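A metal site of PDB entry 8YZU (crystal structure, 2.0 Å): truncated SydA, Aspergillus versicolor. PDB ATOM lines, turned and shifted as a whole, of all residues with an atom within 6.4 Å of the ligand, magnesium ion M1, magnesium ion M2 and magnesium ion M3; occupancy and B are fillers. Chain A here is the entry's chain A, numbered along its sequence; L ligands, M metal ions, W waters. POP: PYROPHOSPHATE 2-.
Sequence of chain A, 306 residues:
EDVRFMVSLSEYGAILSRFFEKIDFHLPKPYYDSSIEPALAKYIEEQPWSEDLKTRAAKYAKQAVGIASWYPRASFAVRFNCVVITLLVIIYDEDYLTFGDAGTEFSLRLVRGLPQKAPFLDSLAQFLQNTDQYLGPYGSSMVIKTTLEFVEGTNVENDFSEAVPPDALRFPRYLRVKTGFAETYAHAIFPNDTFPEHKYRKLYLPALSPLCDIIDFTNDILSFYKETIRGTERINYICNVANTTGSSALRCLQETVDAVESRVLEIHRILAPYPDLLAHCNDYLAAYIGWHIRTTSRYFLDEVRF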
ATOM      1  N   ILE A  90     -18.550   5.319 -11.778  1.00  0.00           N
ATOM      2  CA  ILE A  90     -19.444   4.497 -10.947  1.00  0.00           C
ATOM      3  C   ILE A  90     -20.907   4.734 -11.326  1.00  0.00           C
ATOM      4  O   ILE A  90     -21.699   3.790 -11.418  1.00  0.00           O
ATOM      5  CB  ILE A  90     -19.200   4.785  -9.453  1.00  0.00           C
ATOM      6  CG1 ILE A  90     -17.875   4.205  -8.997  1.00  0.00           C
ATOM      7  CG2 ILE A  90     -20.320   4.152  -8.625  1.00  0.00           C
ATOM      8  CD1 ILE A  90     -17.492   4.640  -7.588  1.00  0.00           C
ATOM      9  N   ASP A  93     -21.263   2.773 -14.619  1.00  0.00           N
ATOM     10  CA  ASP A  93     -21.178   1.325 -14.376  1.00  0.00           C
ATOM     11  C   ASP A  93     -22.474   0.776 -13.785  1.00  0.00           C
ATOM     12  O   ASP A  93     -22.993  -0.266 -14.221  1.00  0.00           O
ATOM     13  CB  ASP A  93     -20.010   1.020 -13.439  1.00  0.00           C
ATOM     14  CG  ASP A  93     -19.412  -0.370 -13.666  1.00  0.00           C
ATOM     15  OD1 ASP A  93     -18.925  -0.645 -14.780  1.00  0.00           O
ATOM     16  OD2 ASP A  93     -19.437  -1.194 -12.731  1.00  0.00           O
ATOM     17  N   GLU A  94     -23.025   1.479 -12.795  1.00  0.00           N
ATOM     18  CA  GLU A  94     -24.272   1.045 -12.173  1.00  0.00           C
ATOM     19  C   GLU A  94     -25.498   1.390 -13.022  1.00  0.00           C
ATOM     20  O   GLU A  94     -26.401   0.566 -13.171  1.00  0.00           O
ATOM     21  CB  GLU A  94     -24.394   1.679 -10.799  1.00  0.00           C
ATOM     22  CG  GLU A  94     -23.232   1.373  -9.870  1.00  0.00           C
ATOM     23  CD  GLU A  94     -23.075  -0.129  -9.629  1.00  0.00           C
ATOM     24  OE1 GLU A  94     -24.066  -0.747  -9.224  1.00  0.00           O
ATOM     25  OE2 GLU A  94     -21.953  -0.681  -9.869  1.00  0.00           O
ATOM     26  N   PHE A 150     -14.652   2.758 -22.362  1.00  0.00           N
ATOM     27  CA  PHE A 150     -15.441   2.377 -21.197  1.00  0.00           C
ATOM     28  C   PHE A 150     -16.936   2.554 -21.453  1.00  0.00           C
ATOM     29  O   PHE A 150     -17.735   1.706 -21.049  1.00  0.00           O
ATOM     30  CB  PHE A 150     -15.026   3.186 -19.965  1.00  0.00           C
ATOM     31  CG  PHE A 150     -16.016   3.096 -18.830  1.00  0.00           C
ATOM     32  CD1 PHE A 150     -16.009   1.997 -17.986  1.00  0.00           C
ATOM     33  CD2 PHE A 150     -16.948   4.115 -18.601  1.00  0.00           C
ATOM     34  CE1 PHE A 150     -16.926   1.891 -16.944  1.00  0.00           C
ATOM     35  CE2 PHE A 150     -17.862   4.000 -17.560  1.00  0.00           C
ATOM     36  CZ  PHE A 150     -17.839   2.895 -16.716  1.00  0.00           C
ATOM     37  N   THR A 154     -19.227  -0.874 -21.498  1.00  0.00           N
ATOM     38  CA  THR A 154     -20.355  -0.997 -20.574  1.00  0.00           C
ATOM     39  C   THR A 154     -21.663  -1.210 -21.333  1.00  0.00           C
ATOM     40  O   THR A 154     -22.539  -1.967 -20.873  1.00  0.00           O
ATOM     41  CB  THR A 154     -20.435   0.256 -19.690  1.00  0.00           C
ATOM     42  OG1 THR A 154     -19.223   0.392 -18.938  1.00  0.00           O
ATOM     43  CG2 THR A 154     -21.685   0.232 -18.724  1.00  0.00           C
ATOM     44  N   GLU A 157     -21.291  -5.096 -23.027  1.00  0.00           N
ATOM     45  CA  GLU A 157     -20.939  -6.180 -22.106  1.00  0.00           C
ATOM     46  C   GLU A 157     -21.946  -7.328 -22.047  1.00  0.00           C
ATOM     47  O   GLU A 157     -21.596  -8.509 -22.205  1.00  0.00           O
ATOM     48  CB  GLU A 157     -20.846  -5.563 -20.709  1.00  0.00           C
ATOM     49  CG  GLU A 157     -19.661  -5.932 -19.955  1.00  0.00           C
ATOM     50  CD  GLU A 157     -19.457  -5.041 -18.776  1.00  0.00           C
ATOM     51  OE1 GLU A 157     -20.177  -4.010 -18.621  1.00  0.00           O
ATOM     52  OE2 GLU A 157     -18.576  -5.402 -17.975  1.00  0.00           O
ATOM     53  N   ARG A 176     -12.064  -6.819 -21.445  1.00  0.00           N
ATOM     54  CA  ARG A 176     -11.630  -6.224 -20.179  1.00  0.00           C
ATOM     55  C   ARG A 176     -10.851  -4.919 -20.385  1.00  0.00           C
ATOM     56  O   ARG A 176     -10.947  -4.010 -19.550  1.00  0.00           O
ATOM     57  CB  ARG A 176     -10.798  -7.201 -19.378  1.00  0.00           C
ATOM     58  CG  ARG A 176     -10.470  -6.665 -17.991  1.00  0.00           C
ATOM     59  CD  ARG A 176     -11.724  -6.088 -17.304  1.00  0.00           C
ATOM     60  NE  ARG A 176     -11.527  -5.891 -15.875  1.00  0.00           N
ATOM     61  CZ  ARG A 176     -12.319  -5.166 -15.092  1.00  0.00           C
ATOM     62  NH1 ARG A 176     -13.347  -4.461 -15.584  1.00  0.00           N
ATOM     63  NH2 ARG A 176     -12.074  -5.135 -13.774  1.00  0.00           N
ATOM     64  N   THR A 179     -13.742  -2.465 -20.712  1.00  0.00           N
ATOM     65  CA  THR A 179     -14.571  -2.173 -19.545  1.00  0.00           C
ATOM     66  C   THR A 179     -13.762  -1.659 -18.351  1.00  0.00           C
ATOM     67  O   THR A 179     -14.358  -1.056 -17.441  1.00  0.00           O
ATOM     68  CB  THR A 179     -15.364  -3.407 -19.078  1.00  0.00           C
ATOM     69  OG1 THR A 179     -14.464  -4.406 -18.582  1.00  0.00           O
ATOM     70  CG2 THR A 179     -16.190  -4.003 -20.215  1.00  0.00           C
ATOM     71  N   GLY A 180     -12.456  -1.890 -18.336  1.00  0.00           N
ATOM     72  CA  GLY A 180     -11.684  -1.678 -17.124  1.00  0.00           C
ATOM     73  C   GLY A 180     -11.347  -0.244 -16.752  1.00  0.00           C
ATOM     74  O   GLY A 180     -11.130   0.049 -15.577  1.00  0.00           O
ATOM     75  N   PHE A 181     -11.222   0.651 -17.737  1.00  0.00           N
ATOM     76  CA  PHE A 181     -10.906   2.066 -17.467  1.00  0.00           C
ATOM     77  C   PHE A 181      -9.508   2.263 -16.856  1.00  0.00           C
ATOM     78  O   PHE A 181      -9.243   3.273 -16.221  1.00  0.00           O
ATOM     79  CB  PHE A 181     -11.978   2.696 -16.547  1.00  0.00           C
ATOM     80  CG  PHE A 181     -12.071   4.183 -16.638  1.00  0.00           C
ATOM     81  CD1 PHE A 181     -12.521   4.791 -17.796  1.00  0.00           C
ATOM     82  CD2 PHE A 181     -11.727   4.975 -15.557  1.00  0.00           C
ATOM     83  CE1 PHE A 181     -12.602   6.177 -17.881  1.00  0.00           C
ATOM     84  CE2 PHE A 181     -11.831   6.363 -15.621  1.00  0.00           C
ATOM     85  CZ  PHE A 181     -12.263   6.957 -16.794  1.00  0.00           C
ATOM     86  N   ASN A 219      -9.048  -5.797  -9.660  1.00  0.00           N
ATOM     87  CA  ASN A 219     -10.488  -5.639  -9.456  1.00  0.00           C
ATOM     88  C   ASN A 219     -11.211  -6.920  -9.800  1.00  0.00           C
ATOM     89  O   ASN A 219     -12.183  -7.293  -9.127  1.00  0.00           O
ATOM     90  CB  ASN A 219     -11.053  -4.484 -10.289  1.00  0.00           C
ATOM     91  CG  ASN A 219     -12.566  -4.419 -10.221  1.00  0.00           C
ATOM     92  OD1 ASN A 219     -13.270  -4.993 -11.063  1.00  0.00           O
ATOM     93  ND2 ASN A 219     -13.081  -3.751  -9.191  1.00  0.00           N
ATOM     94  N   ASP A 220     -10.804  -7.593 -10.868  1.00  0.00           N
ATOM     95  CA  ASP A 220     -11.433  -8.869 -11.203  1.00  0.00           C
ATOM     96  C   ASP A 220     -11.315  -9.847 -10.044  1.00  0.00           C
ATOM     97  O   ASP A 220     -12.307 -10.467  -9.624  1.00  0.00           O
ATOM     98  CB  ASP A 220     -10.830  -9.422 -12.486  1.00  0.00           C
ATOM     99  CG  ASP A 220     -11.321  -8.652 -13.731  1.00  0.00           C
ATOM    100  OD1 ASP A 220     -12.544  -8.396 -13.786  1.00  0.00           O
ATOM    101  OD2 ASP A 220     -10.503  -8.303 -14.629  1.00  0.00           O
ATOM    102  N   SER A 223     -13.417  -8.255  -6.929  1.00  0.00           N
ATOM    103  CA  SER A 223     -14.836  -7.990  -7.120  1.00  0.00           C
ATOM    104  C   SER A 223     -15.564  -9.230  -7.603  1.00  0.00           C
ATOM    105  O   SER A 223     -16.776  -9.154  -7.856  1.00  0.00           O
ATOM    106  CB  SER A 223     -15.070  -6.819  -8.082  1.00  0.00           C
ATOM    107  OG  SER A 223     -14.612  -7.097  -9.403  1.00  0.00           O
ATOM    108  N   PHE A 224     -14.856 -10.360  -7.716  1.00  0.00           N
ATOM    109  CA  PHE A 224     -15.513 -11.610  -8.086  1.00  0.00           C
ATOM    110  C   PHE A 224     -16.560 -12.020  -7.062  1.00  0.00           C
ATOM    111  O   PHE A 224     -17.555 -12.634  -7.436  1.00  0.00           O
ATOM    112  CB  PHE A 224     -14.469 -12.728  -8.264  1.00  0.00           C
ATOM    113  CG  PHE A 224     -15.070 -14.004  -8.776  1.00  0.00           C
ATOM    114  CD1 PHE A 224     -15.331 -14.162 -10.126  1.00  0.00           C
ATOM    115  CD2 PHE A 224     -15.402 -15.041  -7.904  1.00  0.00           C
ATOM    116  CE1 PHE A 224     -15.901 -15.338 -10.616  1.00  0.00           C
ATOM    117  CE2 PHE A 224     -15.972 -16.217  -8.394  1.00  0.00           C
ATOM    118  CZ  PHE A 224     -16.223 -16.361  -9.742  1.00  0.00           C
ATOM    119  N   LYS A 226     -18.612  -9.926  -5.219  1.00  0.00           N
ATOM    120  CA  LYS A 226     -19.853  -9.180  -5.357  1.00  0.00           C
ATOM    121  C   LYS A 226     -20.506  -9.433  -6.712  1.00  0.00           C
ATOM    122  O   LYS A 226     -21.733  -9.349  -6.830  1.00  0.00           O
ATOM    123  CB  LYS A 226     -19.626  -7.671  -5.144  1.00  0.00           C
ATOM    124  CG  LYS A 226     -18.847  -6.983  -6.271  1.00  0.00           C
ATOM    125  CD  LYS A 226     -19.755  -6.174  -7.193  1.00  0.00           C
ATOM    126  CE  LYS A 226     -18.991  -5.186  -8.084  1.00  0.00           C
ATOM    127  NZ  LYS A 226     -19.878  -4.810  -9.238  1.00  0.00           N
ATOM    128  N   GLU A 227     -19.711  -9.757  -7.719  1.00  0.00           N
ATOM    129  CA  GLU A 227     -20.205  -9.945  -9.082  1.00  0.00           C
ATOM    130  C   GLU A 227     -20.817 -11.330  -9.290  1.00  0.00           C
ATOM    131  O   GLU A 227     -21.908 -11.447  -9.855  1.00  0.00           O
ATOM    132  CB  GLU A 227     -19.071  -9.700 -10.089  1.00  0.00           C
ATOM    133  CG  GLU A 227     -18.645  -8.241 -10.160  1.00  0.00           C
ATOM    134  CD  GLU A 227     -17.417  -7.982 -11.009  1.00  0.00           C
ATOM    135  OE1 GLU A 227     -16.880  -8.922 -11.656  1.00  0.00           O
ATOM    136  OE2 GLU A 227     -16.999  -6.799 -11.024  1.00  0.00           O
ATOM    137  N   GLU A 233     -23.565 -11.666 -12.088  1.00  0.00           N
ATOM    138  CA  GLU A 233     -22.792 -11.277 -13.266  1.00  0.00           C
ATOM    139  C   GLU A 233     -21.937 -12.445 -13.742  1.00  0.00           C
ATOM    140  O   GLU A 233     -21.090 -12.947 -12.995  1.00  0.00           O
ATOM    141  CB  GLU A 233     -21.924 -10.071 -12.947  1.00  0.00           C
ATOM    142  CG  GLU A 233     -21.032  -9.642 -14.092  1.00  0.00           C
ATOM    143  CD  GLU A 233     -20.322  -8.328 -13.823  1.00  0.00           C
ATOM    144  OE1 GLU A 233     -20.819  -7.537 -12.996  1.00  0.00           O
ATOM    145  OE2 GLU A 233     -19.284  -8.074 -14.469  1.00  0.00           O
ATOM    146  N   ASN A 236     -18.251 -11.048 -16.686  1.00  0.00           N
ATOM    147  CA  ASN A 236     -16.982 -10.422 -16.307  1.00  0.00           C
ATOM    148  C   ASN A 236     -15.803 -11.227 -16.856  1.00  0.00           C
ATOM    149  O   ASN A 236     -15.951 -12.326 -17.419  1.00  0.00           O
ATOM    150  CB  ASN A 236     -16.892 -10.272 -14.783  1.00  0.00           C
ATOM    151  CG  ASN A 236     -17.167 -11.565 -14.029  1.00  0.00           C
ATOM    152  OD1 ASN A 236     -17.158 -12.651 -14.603  1.00  0.00           O
ATOM    153  ND2 ASN A 236     -17.430 -11.441 -12.725  1.00  0.00           N
ATOM    154  N   TRP A 291      -8.900   0.052  -0.599  1.00  0.00           N
ATOM    155  CA  TRP A 291     -10.191   0.654  -0.940  1.00  0.00           C
ATOM    156  C   TRP A 291     -11.218  -0.416  -1.300  1.00  0.00           C
ATOM    157  O   TRP A 291     -12.398  -0.292  -0.960  1.00  0.00           O
ATOM    158  CB  TRP A 291     -10.011   1.668  -2.064  1.00  0.00           C
ATOM    159  CG  TRP A 291     -11.297   2.271  -2.547  1.00  0.00           C
ATOM    160  CD1 TRP A 291     -11.963   3.350  -2.011  1.00  0.00           C
ATOM    161  CD2 TRP A 291     -12.087   1.839  -3.663  1.00  0.00           C
ATOM    162  NE1 TRP A 291     -13.099   3.617  -2.738  1.00  0.00           N
ATOM    163  CE2 TRP A 291     -13.197   2.690  -3.762  1.00  0.00           C
ATOM    164  CE3 TRP A 291     -11.940   0.807  -4.606  1.00  0.00           C
ATOM    165  CZ2 TRP A 291     -14.179   2.549  -4.738  1.00  0.00           C
ATOM    166  CZ3 TRP A 291     -12.913   0.659  -5.590  1.00  0.00           C
ATOM    167  CH2 TRP A 291     -14.007   1.532  -5.651  1.00  0.00           C
ATOM    168  N   HIS A 292     -10.796  -1.465  -2.014  1.00  0.00           N
ATOM    169  CA  HIS A 292     -11.697  -2.579  -2.305  1.00  0.00           C
ATOM    170  C   HIS A 292     -12.155  -3.254  -1.024  1.00  0.00           C
ATOM    171  O   HIS A 292     -13.335  -3.623  -0.886  1.00  0.00           O
ATOM    172  CB  HIS A 292     -10.996  -3.599  -3.226  1.00  0.00           C
ATOM    173  CG  HIS A 292     -11.073  -3.283  -4.692  1.00  0.00           C
ATOM    174  ND1 HIS A 292     -10.176  -2.443  -5.337  1.00  0.00           N
ATOM    175  CD2 HIS A 292     -11.921  -3.710  -5.660  1.00  0.00           C
ATOM    176  CE1 HIS A 292     -10.482  -2.359  -6.619  1.00  0.00           C
ATOM    177  NE2 HIS A 292     -11.547  -3.117  -6.835  1.00  0.00           N
ATOM    178  N   ARG A 298     -19.775  -1.663  -1.707  1.00  0.00           N
ATOM    179  CA  ARG A 298     -19.643  -2.053  -3.118  1.00  0.00           C
ATOM    180  C   ARG A 298     -19.150  -3.495  -3.294  1.00  0.00           C
ATOM    181  O   ARG A 298     -19.621  -4.188  -4.206  1.00  0.00           O
ATOM    182  CB  ARG A 298     -18.705  -1.081  -3.852  1.00  0.00           C
ATOM    183  CG  ARG A 298     -18.773  -1.140  -5.411  1.00  0.00           C
ATOM    184  CD  ARG A 298     -17.953  -0.055  -6.151  1.00  0.00           C
ATOM    185  NE  ARG A 298     -18.033  -0.250  -7.593  1.00  0.00           N
ATOM    186  CZ  ARG A 298     -19.145  -0.102  -8.308  1.00  0.00           C
ATOM    187  NH1 ARG A 298     -20.250   0.400  -7.760  1.00  0.00           N
ATOM    188  NH2 ARG A 298     -19.167  -0.482  -9.579  1.00  0.00           N
ATOM    189  N   TYR A 299     -18.200  -3.954  -2.472  1.00  0.00           N
ATOM    190  CA  TYR A 299     -17.567  -5.250  -2.720  1.00  0.00           C
ATOM    191  C   TYR A 299     -17.845  -6.297  -1.649  1.00  0.00           C
ATOM    192  O   TYR A 299     -17.613  -7.493  -1.902  1.00  0.00           O
ATOM    193  CB  TYR A 299     -16.038  -5.084  -2.911  1.00  0.00           C
ATOM    194  CG  TYR A 299     -15.731  -4.157  -4.083  1.00  0.00           C
ATOM    195  CD1 TYR A 299     -15.963  -4.569  -5.388  1.00  0.00           C
ATOM    196  CD2 TYR A 299     -15.277  -2.866  -3.877  1.00  0.00           C
ATOM    197  CE1 TYR A 299     -15.740  -3.723  -6.468  1.00  0.00           C
ATOM    198  CE2 TYR A 299     -15.029  -2.003  -4.955  1.00  0.00           C
ATOM    199  CZ  TYR A 299     -15.270  -2.440  -6.248  1.00  0.00           C
ATOM    200  OH  TYR A 299     -15.037  -1.582  -7.313  1.00  0.00           O
HETATM  201  P1  POP L   1     -15.908  -3.295 -13.027  1.00  0.00           P
HETATM  202  O1  POP L   1     -15.754  -4.804 -12.837  1.00  0.00           O
HETATM  203  O2  POP L   1     -17.270  -2.992 -13.662  1.00  0.00           O
HETATM  204  O3  POP L   1     -14.853  -2.734 -13.961  1.00  0.00           O
HETATM  205  O   POP L   1     -15.808  -2.541 -11.619  1.00  0.00           O
HETATM  206  P2  POP L   1     -16.601  -3.058 -10.330  1.00  0.00           P
HETATM  207  O4  POP L   1     -15.941  -4.353  -9.918  1.00  0.00           O
HETATM  208  O5  POP L   1     -18.073  -3.265 -10.637  1.00  0.00           O
HETATM  209  O6  POP L   1     -16.451  -2.008  -9.239  1.00  0.00           O
HETATM  210 MG    MG M   1     -15.298  -5.803 -11.149  1.00  0.00          MG
HETATM  211 MG    MG M   2     -17.919  -2.377 -15.489  1.00  0.00          MG
HETATM  212 MG    MG M   3     -18.904  -3.242 -12.577  1.00  0.00          MG
HETATM  213  O   HOH W   1     -17.405  -4.238 -16.392  1.00  0.00           O
HETATM  214  O   HOH W   2     -20.844  -3.376 -11.793  1.00  0.00           O
HETATM  215  O   HOH W   3     -19.101  -5.234 -12.473  1.00  0.00           O
HETATM  216  O   HOH W   4     -16.572  -6.481 -14.753  1.00  0.00           O
HETATM  217  O   HOH W   5     -14.504  -7.465 -12.168  1.00  0.00           O
HETATM  218  O   HOH W   6     -19.641  -3.466 -14.478  1.00  0.00           O
HETATM  219  O   HOH W   7     -16.318  -1.507 -15.951  1.00  0.00           O
HETATM  220  O   HOH W   8     -18.762  -1.838 -17.438  1.00  0.00           O
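Lys 226 touches magnesium ion M3 (NZ to MG, 3.8 Å). Within 4 Å of magnesium ion M3: Asp 93 and Lys 226.
The side-chain amide nitrogen (ND2) of Asn 219 lies within hydrogen-bond range of a ring nitrogen (NE2) of His 292 (2.9 Å). The side-chain carboxylate of Glu 227 is in hydrogen-bond range of the side-chain amide nitrogen of Asn 236 (2.8 Å). The side-chain amide nitrogen (ND2) of Asn 219 lies within hydrogen-bond range of the side-chain hydroxyl (OH) of Tyr 299 (3.5 Å). NE of Arg 176 is in salt-bridge range of OD2 of Asp 220 (2.9 Å). NH2 of Arg 176 sits close to OD1 of Asn 219, 3.0 Å away. The side-chain carboxylate (OD2) of Asp 93 sits close to the guanidinium group (NH2) of Arg 298 (3.2 Å). The backbone NH of Glu 233 is in hydrogen-bond range of the backbone carbonyl oxygen of Glu 227 (2.8 Å). OE2 of Glu 227 sits close to NZ of Lys 226 (3.9 Å).
Magnesium ion M3 is bound by an oxygen (O2) of the ligand (2.0 Å), water W3 (2.0 Å), water W6 (2.1 Å), water W2 (2.1 Å), an oxygen (O5) of the ligand (2.1 Å) and the side-chain carboxylate of Asp 93 (2.1 Å). Magnesium ion M3 has six donor atoms within binding distance.
Water W5 bridges the side-chain carboxylate (OD1) of Asp 220 (2.7 Å) and the side-chain carboxylate (OE1) of Glu 227 (2.8 Å). Water W7 bridges the backbone carbonyl oxygen of Thr 179 and an oxygen (O3) of the ligand. Water W8 lies within hydrogen-bond range of the side-chain hydroxyl (OG1) of Thr 154 and the side-chain carboxylate (OE1) of Glu 157. Water W3 bridges OE1 of Glu 233 (2.9 Å) and NZ of Lys 226 (3.4 Å). Water W2 lies within hydrogen-bond range of NZ of Lys 226 (3.1 Å) and OE2 of Glu 94 (3.5 Å).
Of the 22 residues printed, 3 come within 4 Å of magnesium ion M1. The nearest printed residue that does not touch magnesium ion M1 is Arg 176 (4.2 Å).
An oxygen (O5) of the ligand lies close to the side-chain amino group (NZ) of Lys 226. The guanidinium group (NE) of Arg 298 lies within salt-bridge range of an oxygen (O6) of the ligand (2.9 Å). The guanidinium group (NH1) of Arg 176 lies within salt-bridge range of an oxygen (O3) of the ligand (2.8 Å). An oxygen (O6) of the ligand sits at hydrogen-bond distance from the side-chain hydroxyl (OH) of Tyr 299, at 2.4 Å.
OE2 of Glu 157 touches magnesium ion M2 (3.97 Å). The nearest printed residue that does not touch magnesium ion M2 is Thr 179 (4.3 Å).
Residues that only touch the ligand: Thr 179. Hydrophobic or aromatic side chains that line the ligand: Tyr 299. Within 4 Å of the ligand: Asp 93, Arg 176, Thr 179, Asn 219, Ser 223, Lys 226, Glu 227, Arg 298 and Tyr 299.
Magnesium ion M1 is bound by OE2 of Glu 227 (2.0 Å), O4 of the ligand (2.0 Å), O1 of the ligand (2.0 Å), water W5 (2.1 Å), OD1 of Asn 219 (2.2 Å) and OG of Ser 223 (2.3 Å).
Magnesium ion M2 is bound by water W7, an oxygen (O2) of the ligand, the side-chain carboxylate of Asp 93, water W1, water W8 and water W6.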
